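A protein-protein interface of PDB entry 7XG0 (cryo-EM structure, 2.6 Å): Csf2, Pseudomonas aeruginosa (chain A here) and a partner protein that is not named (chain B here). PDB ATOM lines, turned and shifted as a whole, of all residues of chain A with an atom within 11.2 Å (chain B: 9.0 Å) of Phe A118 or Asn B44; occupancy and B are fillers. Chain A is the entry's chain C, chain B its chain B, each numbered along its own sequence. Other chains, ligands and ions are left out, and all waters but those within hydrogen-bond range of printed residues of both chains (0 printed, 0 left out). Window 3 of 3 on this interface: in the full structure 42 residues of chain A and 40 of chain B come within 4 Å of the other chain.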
ATOM      1  N   VAL A 114      23.809  18.087 -33.009  1.00  0.00           N
ATOM      2  CA  VAL A 114      24.270  19.325 -33.646  1.00  0.00           C
ATOM      3  C   VAL A 114      25.236  20.046 -32.715  1.00  0.00           C
ATOM      4  O   VAL A 114      24.876  20.343 -31.558  1.00  0.00           O
ATOM      5  CB  VAL A 114      23.076  20.224 -34.005  1.00  0.00           C
ATOM      6  CG1 VAL A 114      23.561  21.576 -34.501  1.00  0.00           C
ATOM      7  CG2 VAL A 114      22.213  19.550 -35.053  1.00  0.00           C
ATOM      8  N   PRO A 115      26.462  20.335 -33.145  1.00  0.00           N
ATOM      9  CA  PRO A 115      27.355  21.159 -32.328  1.00  0.00           C
ATOM     10  C   PRO A 115      26.883  22.601 -32.275  1.00  0.00           C
ATOM     11  O   PRO A 115      26.396  23.164 -33.258  1.00  0.00           O
ATOM     12  CB  PRO A 115      28.704  21.039 -33.049  1.00  0.00           C
ATOM     13  CG  PRO A 115      28.342  20.760 -34.467  1.00  0.00           C
ATOM     14  CD  PRO A 115      27.077  19.945 -34.426  1.00  0.00           C
ATOM     15  N   SER A 116      27.023  23.194 -31.094  1.00  0.00           N
ATOM     16  CA  SER A 116      26.534  24.545 -30.862  1.00  0.00           C
ATOM     17  C   SER A 116      27.629  25.378 -30.220  1.00  0.00           C
ATOM     18  O   SER A 116      28.137  25.025 -29.151  1.00  0.00           O
ATOM     19  CB  SER A 116      25.285  24.531 -29.975  1.00  0.00           C
ATOM     20  OG  SER A 116      24.247  23.772 -30.569  1.00  0.00           O
ATOM     21  N   SER A 117      27.990  26.478 -30.876  1.00  0.00           N
ATOM     22  CA  SER A 117      28.904  27.442 -30.291  1.00  0.00           C
ATOM     23  C   SER A 117      28.188  28.250 -29.214  1.00  0.00           C
ATOM     24  O   SER A 117      26.960  28.247 -29.113  1.00  0.00           O
ATOM     25  CB  SER A 117      29.472  28.374 -31.362  1.00  0.00           C
ATOM     26  OG  SER A 117      28.565  29.417 -31.670  1.00  0.00           O
ATOM     27  N   PHE A 118      28.981  28.950 -28.401  1.00  0.00           N
ATOM     28  CA  PHE A 118      28.426  29.682 -27.267  1.00  0.00           C
ATOM     29  C   PHE A 118      27.640  30.906 -27.724  1.00  0.00           C
ATOM     30  O   PHE A 118      26.682  31.322 -27.060  1.00  0.00           O
ATOM     31  CB  PHE A 118      29.552  30.074 -26.314  1.00  0.00           C
ATOM     32  CG  PHE A 118      30.492  28.946 -26.008  1.00  0.00           C
ATOM     33  CD1 PHE A 118      30.012  27.745 -25.504  1.00  0.00           C
ATOM     34  CD2 PHE A 118      31.851  29.072 -26.252  1.00  0.00           C
ATOM     35  CE1 PHE A 118      30.872  26.697 -25.232  1.00  0.00           C
ATOM     36  CE2 PHE A 118      32.717  28.028 -25.983  1.00  0.00           C
ATOM     37  CZ  PHE A 118      32.226  26.839 -25.474  1.00  0.00           C
ATOM     38  N   ASP A 119      28.025  31.487 -28.863  1.00  0.00           N
ATOM     39  CA  ASP A 119      27.307  32.640 -29.400  1.00  0.00           C
ATOM     40  C   ASP A 119      25.919  32.247 -29.893  1.00  0.00           C
ATOM     41  O   ASP A 119      24.927  32.926 -29.598  1.00  0.00           O
ATOM     42  CB  ASP A 119      28.120  33.278 -30.525  1.00  0.00           C
ATOM     43  CG  ASP A 119      29.529  33.636 -30.094  1.00  0.00           C
ATOM     44  OD1 ASP A 119      29.837  33.502 -28.892  1.00  0.00           O
ATOM     45  OD2 ASP A 119      30.330  34.049 -30.960  1.00  0.00           O
ATOM     46  N   GLU A 120      25.825  31.140 -30.637  1.00  0.00           N
ATOM     47  CA  GLU A 120      24.515  30.709 -31.111  1.00  0.00           C
ATOM     48  C   GLU A 120      23.686  30.103 -29.986  1.00  0.00           C
ATOM     49  O   GLU A 120      22.455  30.172 -30.032  1.00  0.00           O
ATOM     50  CB  GLU A 120      24.654  29.736 -32.285  1.00  0.00           C
ATOM     51  CG  GLU A 120      25.403  28.455 -31.999  1.00  0.00           C
ATOM     52  CD  GLU A 120      25.707  27.675 -33.264  1.00  0.00           C
ATOM     53  OE1 GLU A 120      24.995  27.879 -34.270  1.00  0.00           O
ATOM     54  OE2 GLU A 120      26.659  26.868 -33.258  1.00  0.00           O
ATOM     55  N   ILE A 121      24.339  29.557 -28.953  1.00  0.00           N
ATOM     56  CA  ILE A 121      23.633  29.157 -27.735  1.00  0.00           C
ATOM     57  C   ILE A 121      23.022  30.377 -27.051  1.00  0.00           C
ATOM     58  O   ILE A 121      21.870  30.340 -26.598  1.00  0.00           O
ATOM     59  CB  ILE A 121      24.583  28.377 -26.800  1.00  0.00           C
ATOM     60  CG1 ILE A 121      24.649  26.906 -27.216  1.00  0.00           C
ATOM     61  CG2 ILE A 121      24.177  28.481 -25.328  1.00  0.00           C
ATOM     62  CD1 ILE A 121      25.587  26.069 -26.372  1.00  0.00           C
ATOM     63  N   ALA A 122      23.771  31.486 -26.996  1.00  0.00           N
ATOM     64  CA  ALA A 122      23.258  32.710 -26.386  1.00  0.00           C
ATOM     65  C   ALA A 122      22.111  33.313 -27.189  1.00  0.00           C
ATOM     66  O   ALA A 122      21.135  33.801 -26.609  1.00  0.00           O
ATOM     67  CB  ALA A 122      24.380  33.731 -26.233  1.00  0.00           C
ATOM     68  N   THR A 123      22.217  33.307 -28.521  1.00  0.00           N
ATOM     69  CA  THR A 123      21.132  33.847 -29.338  1.00  0.00           C
ATOM     70  C   THR A 123      19.909  32.936 -29.314  1.00  0.00           C
ATOM     71  O   THR A 123      18.771  33.413 -29.399  1.00  0.00           O
ATOM     72  CB  THR A 123      21.594  34.078 -30.779  1.00  0.00           C
ATOM     73  OG1 THR A 123      21.981  32.832 -31.371  1.00  0.00           O
ATOM     74  CG2 THR A 123      22.751  35.066 -30.830  1.00  0.00           C
ATOM     75  N   MET A 124      20.121  31.624 -29.193  1.00  0.00           N
ATOM     76  CA  MET A 124      19.000  30.695 -29.153  1.00  0.00           C
ATOM     77  C   MET A 124      18.309  30.720 -27.796  1.00  0.00           C
ATOM     78  O   MET A 124      17.090  30.537 -27.712  1.00  0.00           O
ATOM     79  CB  MET A 124      19.492  29.292 -29.497  1.00  0.00           C
ATOM     80  CG  MET A 124      19.328  28.954 -30.964  1.00  0.00           C
ATOM     81  SD  MET A 124      20.577  27.803 -31.556  1.00  0.00           S
ATOM     82  CE  MET A 124      20.547  28.154 -33.311  1.00  0.00           C
ATOM     83  N   ARG A 125      19.065  30.954 -26.723  1.00  0.00           N
ATOM     84  CA  ARG A 125      18.459  31.124 -25.409  1.00  0.00           C
ATOM     85  C   ARG A 125      17.830  32.500 -25.234  1.00  0.00           C
ATOM     86  O   ARG A 125      17.042  32.686 -24.301  1.00  0.00           O
ATOM     87  CB  ARG A 125      19.492  30.869 -24.309  1.00  0.00           C
ATOM     88  CG  ARG A 125      19.843  29.397 -24.129  1.00  0.00           C
ATOM     89  CD  ARG A 125      20.593  29.142 -22.830  1.00  0.00           C
ATOM     90  NE  ARG A 125      19.705  28.705 -21.758  1.00  0.00           N
ATOM     91  CZ  ARG A 125      19.849  29.037 -20.482  1.00  0.00           C
ATOM     92  NH1 ARG A 125      20.843  29.810 -20.077  1.00  0.00           N
ATOM     93  NH2 ARG A 125      18.976  28.579 -19.590  1.00  0.00           N
ATOM     94  N   ALA A 126      18.155  33.457 -26.101  1.00  0.00           N
ATOM     95  CA  ALA A 126      17.488  34.751 -26.129  1.00  0.00           C
ATOM     96  C   ALA A 126      16.329  34.789 -27.115  1.00  0.00           C
ATOM     97  O   ALA A 126      15.677  35.832 -27.243  1.00  0.00           O
ATOM     98  CB  ALA A 126      18.491  35.858 -26.468  1.00  0.00           C
ATOM     99  N   HIS A 127      16.076  33.692 -27.825  1.00  0.00           N
ATOM    100  CA  HIS A 127      14.899  33.593 -28.674  1.00  0.00           C
ATOM    101  C   HIS A 127      13.646  33.548 -27.799  1.00  0.00           C
ATOM    102  O   HIS A 127      13.698  33.013 -26.686  1.00  0.00           O
ATOM    103  CB  HIS A 127      14.991  32.341 -29.550  1.00  0.00           C
ATOM    104  CG  HIS A 127      13.993  32.296 -30.664  1.00  0.00           C
ATOM    105  ND1 HIS A 127      12.764  31.684 -30.540  1.00  0.00           N
ATOM    106  CD2 HIS A 127      14.043  32.784 -31.926  1.00  0.00           C
ATOM    107  CE1 HIS A 127      12.099  31.799 -31.675  1.00  0.00           C
ATOM    108  NE2 HIS A 127      12.853  32.462 -32.534  1.00  0.00           N
ATOM    109  N   ARG A 138      20.054  20.174 -30.757  1.00  0.00           N
ATOM    110  CA  ARG A 138      21.135  20.874 -30.071  1.00  0.00           C
ATOM    111  C   ARG A 138      21.148  20.626 -28.570  1.00  0.00           C
ATOM    112  O   ARG A 138      22.097  21.055 -27.902  1.00  0.00           O
ATOM    113  CB  ARG A 138      21.055  22.376 -30.338  1.00  0.00           C
ATOM    114  CG  ARG A 138      21.200  22.749 -31.798  1.00  0.00           C
ATOM    115  CD  ARG A 138      21.185  24.251 -31.962  1.00  0.00           C
ATOM    116  NE  ARG A 138      21.184  24.658 -33.362  1.00  0.00           N
ATOM    117  CZ  ARG A 138      22.256  25.080 -34.019  1.00  0.00           C
ATOM    118  NH1 ARG A 138      23.439  25.163 -33.433  1.00  0.00           N
ATOM    119  NH2 ARG A 138      22.136  25.433 -35.295  1.00  0.00           N
ATOM    120  N   LEU A 140      19.512  21.828 -26.087  1.00  0.00           N
ATOM    121  CA  LEU A 140      19.695  23.085 -25.372  1.00  0.00           C
ATOM    122  C   LEU A 140      18.845  23.139 -24.106  1.00  0.00           C
ATOM    123  O   LEU A 140      17.726  22.622 -24.064  1.00  0.00           O
ATOM    124  CB  LEU A 140      19.347  24.257 -26.296  1.00  0.00           C
ATOM    125  CG  LEU A 140      19.627  25.685 -25.829  1.00  0.00           C
ATOM    126  CD1 LEU A 140      21.089  26.033 -26.052  1.00  0.00           C
ATOM    127  CD2 LEU A 140      18.723  26.668 -26.555  1.00  0.00           C
ATOM    128  N   GLU A 141      19.395  23.764 -23.064  1.00  0.00           N
ATOM    129  CA  GLU A 141      18.684  23.971 -21.809  1.00  0.00           C
ATOM    130  C   GLU A 141      17.797  25.203 -21.910  1.00  0.00           C
ATOM    131  O   GLU A 141      18.261  26.283 -22.286  1.00  0.00           O
ATOM    132  CB  GLU A 141      19.666  24.124 -20.646  1.00  0.00           C
ATOM    133  CG  GLU A 141      18.992  24.307 -19.295  1.00  0.00           C
ATOM    134  CD  GLU A 141      19.960  24.193 -18.132  1.00  0.00           C
ATOM    135  OE1 GLU A 141      20.941  23.429 -18.242  1.00  0.00           O
ATOM    136  OE2 GLU A 141      19.736  24.869 -17.106  1.00  0.00           O
ATOM    137  N   ARG A 143      15.145  28.241 -20.543  1.00  0.00           N
ATOM    138  CA  ARG A 143      15.068  29.194 -19.443  1.00  0.00           C
ATOM    139  C   ARG A 143      13.913  28.902 -18.495  1.00  0.00           C
ATOM    140  O   ARG A 143      13.820  29.542 -17.443  1.00  0.00           O
ATOM    141  CB  ARG A 143      14.914  30.612 -19.994  1.00  0.00           C
ATOM    142  CG  ARG A 143      16.071  31.103 -20.849  1.00  0.00           C
ATOM    143  CD  ARG A 143      16.505  32.496 -20.447  1.00  0.00           C
ATOM    144  NE  ARG A 143      17.545  33.020 -21.322  1.00  0.00           N
ATOM    145  CZ  ARG A 143      18.839  33.035 -21.031  1.00  0.00           C
ATOM    146  NH1 ARG A 143      19.294  32.554 -19.886  1.00  0.00           N
ATOM    147  NH2 ARG A 143      19.695  33.547 -21.910  1.00  0.00           N
ATOM    148  N   ARG B  31      28.013  28.440 -10.179  1.00  0.00           N
ATOM    149  CA  ARG B  31      28.985  29.447 -10.592  1.00  0.00           C
ATOM    150  C   ARG B  31      28.842  29.768 -12.077  1.00  0.00           C
ATOM    151  O   ARG B  31      29.029  30.917 -12.489  1.00  0.00           O
ATOM    152  CB  ARG B  31      30.399  28.963 -10.267  1.00  0.00           C
ATOM    153  CG  ARG B  31      31.515  29.922 -10.647  1.00  0.00           C
ATOM    154  CD  ARG B  31      31.305  31.314 -10.074  1.00  0.00           C
ATOM    155  NE  ARG B  31      32.410  32.203 -10.405  1.00  0.00           N
ATOM    156  CZ  ARG B  31      32.297  33.297 -11.147  1.00  0.00           C
ATOM    157  NH1 ARG B  31      31.133  33.671 -11.652  1.00  0.00           N
ATOM    158  NH2 ARG B  31      33.378  34.032 -11.389  1.00  0.00           N
ATOM    159  N   VAL B  32      28.490  28.768 -12.890  1.00  0.00           N
ATOM    160  CA  VAL B  32      28.218  28.998 -14.308  1.00  0.00           C
ATOM    161  C   VAL B  32      26.972  29.863 -14.482  1.00  0.00           C
ATOM    162  O   VAL B  32      26.949  30.777 -15.315  1.00  0.00           O
ATOM    163  CB  VAL B  32      28.111  27.644 -15.040  1.00  0.00           C
ATOM    164  CG1 VAL B  32      27.311  27.745 -16.334  1.00  0.00           C
ATOM    165  CG2 VAL B  32      29.501  27.109 -15.335  1.00  0.00           C
ATOM    166  N   ALA B  35      27.986  33.346 -13.548  1.00  0.00           N
ATOM    167  CA  ALA B  35      28.779  33.933 -14.623  1.00  0.00           C
ATOM    168  C   ALA B  35      27.904  34.312 -15.810  1.00  0.00           C
ATOM    169  O   ALA B  35      28.197  35.276 -16.525  1.00  0.00           O
ATOM    170  CB  ALA B  35      29.872  32.959 -15.052  1.00  0.00           C
ATOM    171  N   ARG B  36      26.827  33.556 -16.039  1.00  0.00           N
ATOM    172  CA  ARG B  36      25.834  33.961 -17.027  1.00  0.00           C
ATOM    173  C   ARG B  36      25.078  35.200 -16.572  1.00  0.00           C
ATOM    174  O   ARG B  36      24.618  35.987 -17.406  1.00  0.00           O
ATOM    175  CB  ARG B  36      24.860  32.814 -17.302  1.00  0.00           C
ATOM    176  CG  ARG B  36      25.451  31.664 -18.103  1.00  0.00           C
ATOM    177  CD  ARG B  36      24.405  30.590 -18.367  1.00  0.00           C
ATOM    178  NE  ARG B  36      24.986  29.258 -18.488  1.00  0.00           N
ATOM    179  CZ  ARG B  36      25.539  28.773 -19.592  1.00  0.00           C
ATOM    180  NH1 ARG B  36      25.605  29.486 -20.704  1.00  0.00           N
ATOM    181  NH2 ARG B  36      26.032  27.537 -19.581  1.00  0.00           N
ATOM    182  N   HIS B  39      28.327  38.112 -17.047  1.00  0.00           N
ATOM    183  CA  HIS B  39      28.927  38.300 -18.364  1.00  0.00           C
ATOM    184  C   HIS B  39      28.028  37.815 -19.501  1.00  0.00           C
ATOM    185  O   HIS B  39      28.504  37.583 -20.615  1.00  0.00           O
ATOM    186  CB  HIS B  39      30.283  37.601 -18.435  1.00  0.00           C
ATOM    187  CG  HIS B  39      30.997  37.531 -17.121  1.00  0.00           C
ATOM    188  ND1 HIS B  39      31.292  38.650 -16.372  1.00  0.00           N
ATOM    189  CD2 HIS B  39      31.472  36.474 -16.421  1.00  0.00           C
ATOM    190  CE1 HIS B  39      31.922  38.286 -15.269  1.00  0.00           C
ATOM    191  NE2 HIS B  39      32.042  36.971 -15.273  1.00  0.00           N
ATOM    192  N   GLY B  40      26.735  37.654 -19.240  1.00  0.00           N
ATOM    193  CA  GLY B  40      25.819  37.248 -20.289  1.00  0.00           C
ATOM    194  C   GLY B  40      25.909  35.763 -20.613  1.00  0.00           C
ATOM    195  O   GLY B  40      26.677  35.004 -20.028  1.00  0.00           O
ATOM    196  N   ASP B  41      25.102  35.362 -21.599  1.00  0.00           N
ATOM    197  CA  ASP B  41      24.941  33.953 -21.938  1.00  0.00           C
ATOM    198  C   ASP B  41      25.986  33.480 -22.948  1.00  0.00           C
ATOM    199  O   ASP B  41      26.173  32.272 -23.114  1.00  0.00           O
ATOM    200  CB  ASP B  41      23.519  33.729 -22.490  1.00  0.00           C
ATOM    201  CG  ASP B  41      22.971  32.313 -22.242  1.00  0.00           C
ATOM    202  OD1 ASP B  41      23.699  31.309 -22.342  1.00  0.00           O
ATOM    203  OD2 ASP B  41      21.764  32.208 -21.941  1.00  0.00           O
ATOM    204  N   ALA B  42      26.715  34.397 -23.578  1.00  0.00           N
ATOM    205  CA  ALA B  42      27.696  34.037 -24.602  1.00  0.00           C
ATOM    206  C   ALA B  42      29.068  33.754 -24.001  1.00  0.00           C
ATOM    207  O   ALA B  42      30.071  34.353 -24.385  1.00  0.00           O
ATOM    208  CB  ALA B  42      27.779  35.139 -25.651  1.00  0.00           C
ATOM    209  N   ILE B  43      29.118  32.831 -23.045  1.00  0.00           N
ATOM    210  CA  ILE B  43      30.355  32.466 -22.373  1.00  0.00           C
ATOM    211  C   ILE B  43      30.646  30.988 -22.606  1.00  0.00           C
ATOM    212  O   ILE B  43      29.768  30.192 -22.958  1.00  0.00           O
ATOM    213  CB  ILE B  43      30.311  32.783 -20.859  1.00  0.00           C
ATOM    214  CG1 ILE B  43      29.445  31.758 -20.117  1.00  0.00           C
ATOM    215  CG2 ILE B  43      29.845  34.213 -20.602  1.00  0.00           C
ATOM    216  CD1 ILE B  43      29.330  32.003 -18.636  1.00  0.00           C
ATOM    217  N   ASN B  44      31.917  30.630 -22.433  1.00  0.00           N
ATOM    218  CA  ASN B  44      32.305  29.236 -22.281  1.00  0.00           C
ATOM    219  C   ASN B  44      32.034  28.864 -20.832  1.00  0.00           C
ATOM    220  O   ASN B  44      32.574  29.522 -19.928  1.00  0.00           O
ATOM    221  CB  ASN B  44      33.777  29.042 -22.623  1.00  0.00           C
ATOM    222  CG  ASN B  44      34.187  27.575 -22.723  1.00  0.00           C
ATOM    223  OD1 ASN B  44      33.401  26.663 -22.468  1.00  0.00           O
ATOM    224  ND2 ASN B  44      35.437  27.351 -23.103  1.00  0.00           N
ATOM    225  N   PRO B  45      31.192  27.866 -20.554  1.00  0.00           N
ATOM    226  CA  PRO B  45      31.004  27.432 -19.159  1.00  0.00           C
ATOM    227  C   PRO B  45      32.245  26.815 -18.535  1.00  0.00           C
ATOM    228  O   PRO B  45      32.373  26.833 -17.306  1.00  0.00           O
ATOM    229  CB  PRO B  45      29.861  26.411 -19.257  1.00  0.00           C
ATOM    230  CG  PRO B  45      29.215  26.665 -20.588  1.00  0.00           C
ATOM    231  CD  PRO B  45      30.314  27.132 -21.481  1.00  0.00           C
ATOM    232  N   ARG B  46      33.170  26.295 -19.342  1.00  0.00           N
ATOM    233  CA  ARG B  46      34.329  25.576 -18.831  1.00  0.00           C
ATOM    234  C   ARG B  46      35.418  26.487 -18.280  1.00  0.00           C
ATOM    235  O   ARG B  46      36.377  25.982 -17.687  1.00  0.00           O
ATOM    236  CB  ARG B  46      34.903  24.682 -19.929  1.00  0.00           C
ATOM    237  CG  ARG B  46      33.846  23.832 -20.608  1.00  0.00           C
ATOM    238  CD  ARG B  46      34.196  22.360 -20.548  1.00  0.00           C
ATOM    239  NE  ARG B  46      33.079  21.518 -20.959  1.00  0.00           N
ATOM    240  CZ  ARG B  46      33.205  20.279 -21.409  1.00  0.00           C
ATOM    241  NH1 ARG B  46      34.392  19.709 -21.540  1.00  0.00           N
ATOM    242  NH2 ARG B  46      32.114  19.594 -21.739  1.00  0.00           N
ATOM    243  N   ASP B  47      35.310  27.804 -18.461  1.00  0.00           N
ATOM    244  CA  ASP B  47      36.306  28.690 -17.871  1.00  0.00           C
ATOM    245  C   ASP B  47      35.973  29.043 -16.427  1.00  0.00           C
ATOM    246  O   ASP B  47      36.821  29.605 -15.724  1.00  0.00           O
ATOM    247  CB  ASP B  47      36.443  29.978 -18.687  1.00  0.00           C
ATOM    248  CG  ASP B  47      36.559  29.724 -20.176  1.00  0.00           C
ATOM    249  OD1 ASP B  47      37.086  28.662 -20.568  1.00  0.00           O
ATOM    250  OD2 ASP B  47      36.139  30.604 -20.956  1.00  0.00           O
ATOM    251  N   TYR B  48      34.762  28.725 -15.961  1.00  0.00           N
ATOM    252  CA  TYR B  48      34.300  29.246 -14.684  1.00  0.00           C
ATOM    253  C   TYR B  48      33.833  28.197 -13.688  1.00  0.00           C
ATOM    254  O   TYR B  48      33.802  28.501 -12.492  1.00  0.00           O
ATOM    255  CB  TYR B  48      33.157  30.273 -14.853  1.00  0.00           C
ATOM    256  CG  TYR B  48      33.372  31.418 -15.839  1.00  0.00           C
ATOM    257  CD1 TYR B  48      33.377  31.218 -17.222  1.00  0.00           C
ATOM    258  CD2 TYR B  48      33.420  32.727 -15.379  1.00  0.00           C
ATOM    259  CE1 TYR B  48      33.541  32.273 -18.097  1.00  0.00           C
ATOM    260  CE2 TYR B  48      33.587  33.788 -16.245  1.00  0.00           C
ATOM    261  CZ  TYR B  48      33.638  33.556 -17.603  1.00  0.00           C
ATOM    262  OH  TYR B  48      33.791  34.615 -18.467  1.00  0.00           O
ATOM    263  N   HIS B  49      33.488  26.980 -14.118  1.00  0.00           N
ATOM    264  CA  HIS B  49      33.001  26.026 -13.126  1.00  0.00           C
ATOM    265  C   HIS B  49      34.121  25.415 -12.290  1.00  0.00           C
ATOM    266  O   HIS B  49      33.826  24.688 -11.337  1.00  0.00           O
ATOM    267  CB  HIS B  49      32.150  24.922 -13.774  1.00  0.00           C
ATOM    268  CG  HIS B  49      32.866  24.089 -14.793  1.00  0.00           C
ATOM    269  ND1 HIS B  49      33.843  23.174 -14.463  1.00  0.00           N
ATOM    270  CD2 HIS B  49      32.701  23.992 -16.133  1.00  0.00           C
ATOM    271  CE1 HIS B  49      34.274  22.576 -15.560  1.00  0.00           C
ATOM    272  NE2 HIS B  49      33.598  23.055 -16.587  1.00  0.00           N
ATOM    273  N   TYR B  50      35.385  25.674 -12.625  1.00  0.00           N
ATOM    274  CA  TYR B  50      36.492  25.350 -11.737  1.00  0.00           C
ATOM    275  C   TYR B  50      36.858  26.492 -10.796  1.00  0.00           C
ATOM    276  O   TYR B  50      37.677  26.287  -9.893  1.00  0.00           O
ATOM    277  CB  TYR B  50      37.729  24.938 -12.543  1.00  0.00           C
ATOM    278  CG  TYR B  50      37.612  23.582 -13.200  1.00  0.00           C
ATOM    279  CD1 TYR B  50      36.683  22.651 -12.753  1.00  0.00           C
ATOM    280  CD2 TYR B  50      38.440  23.229 -14.259  1.00  0.00           C
ATOM    281  CE1 TYR B  50      36.575  21.412 -13.346  1.00  0.00           C
ATOM    282  CE2 TYR B  50      38.340  21.987 -14.859  1.00  0.00           C
ATOM    283  CZ  TYR B  50      37.405  21.083 -14.398  1.00  0.00           C
ATOM    284  OH  TYR B  50      37.298  19.846 -14.990  1.00  0.00           O
ATOM    285  N   PRO B 205      32.156  18.716 -15.810  1.00  0.00           N
ATOM    286  CA  PRO B 205      30.935  18.066 -16.297  1.00  0.00           C
ATOM    287  C   PRO B 205      31.019  16.562 -16.114  1.00  0.00           C
ATOM    288  O   PRO B 205      31.731  15.878 -16.856  1.00  0.00           O
ATOM    289  CB  PRO B 205      30.890  18.455 -17.783  1.00  0.00           C
ATOM    290  CG  PRO B 205      31.988  19.474 -17.978  1.00  0.00           C
ATOM    291  CD  PRO B 205      32.993  19.204 -16.916  1.00  0.00           C
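The side-chain carboxylate (OD2) of Asp B41 is in salt-bridge range of the guanidinium group (NH2) of Arg A143, at 2.5 Å.
OD2 of Asp B41 lies within salt-bridge range of NH1 of Arg A125.
The backbone NH of Arg B46 lies within hydrogen-bond range of the side-chain amide oxygen of Asn B44, at 3.2 Å.
OD1 of Asp B47 sits at hydrogen-bond distance from ND2 of Asn B44, at 3.3 Å.
The guanidinium group (NE) of Arg A125 lies within hydrogen-bond range of the backbone carbonyl oxygen (O) of Glu A141 (2.9 Å).
OD1 of Asp B41 is in salt-bridge range of NH1 of Arg B36 (3.1 Å).
The backbone carbonyl oxygen (O) of Arg A125 sits at hydrogen-bond distance from the guanidinium group (NE) of Arg A143 (3.0 Å).
Among the printed residues, pairs that only touch across the chains: Phe A118 with Ala B42 (3.8 Å), Phe A118 with Ile B43 (3.4 Å), Phe A118 with Asn B44 (3.2 Å), Phe A118 with Pro B45 (3.8 Å), Ala A122 with Asp B41 (3.7 Å) and Ala A122 with Ala B42 (3.6 Å).
No residue of chain B comes within 4 Å of Ser A117.
Of chain B, only Ala B42 (3.8 Å), Ile B43 (3.4 Å), Asn B44 (3.2 Å) and Pro B45 (3.8 Å) come within 4 Å of Phe A118.
No residue of chain B comes within 4 Å of Ile A121.
Of the printed residues of chain B, Ala A122 touches Asp B41 (3.7 Å) and Ala B42 (3.6 Å).
Of the printed residues of chain A, Asp B41 touches Ala A122, Arg A125 and Arg A143.
Ala B42 touches just these residues of chain A: Phe A118 and Ala A122.
Asn B44 touches just one residue of chain A: Phe A118 (3.2 Å).
No residue of chain A comes within 4 Å of Asp B47.
The nearest residue of chain B that does not touch Phe A118 is Asp B41 (4.1 Å).
The nearest printed residue of chain A that does not touch Asp B41 is Phe A118 (4.1 Å).
Of the 18 printed residues of chain A, 4 touch a printed residue of chain B.
Hydrophobic or aromatic side chains of chain A within 4 Å of the printed part of chain B: Phe A118 and Ala A122.
Among the printed residues, 8 pairs touch across the chains.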
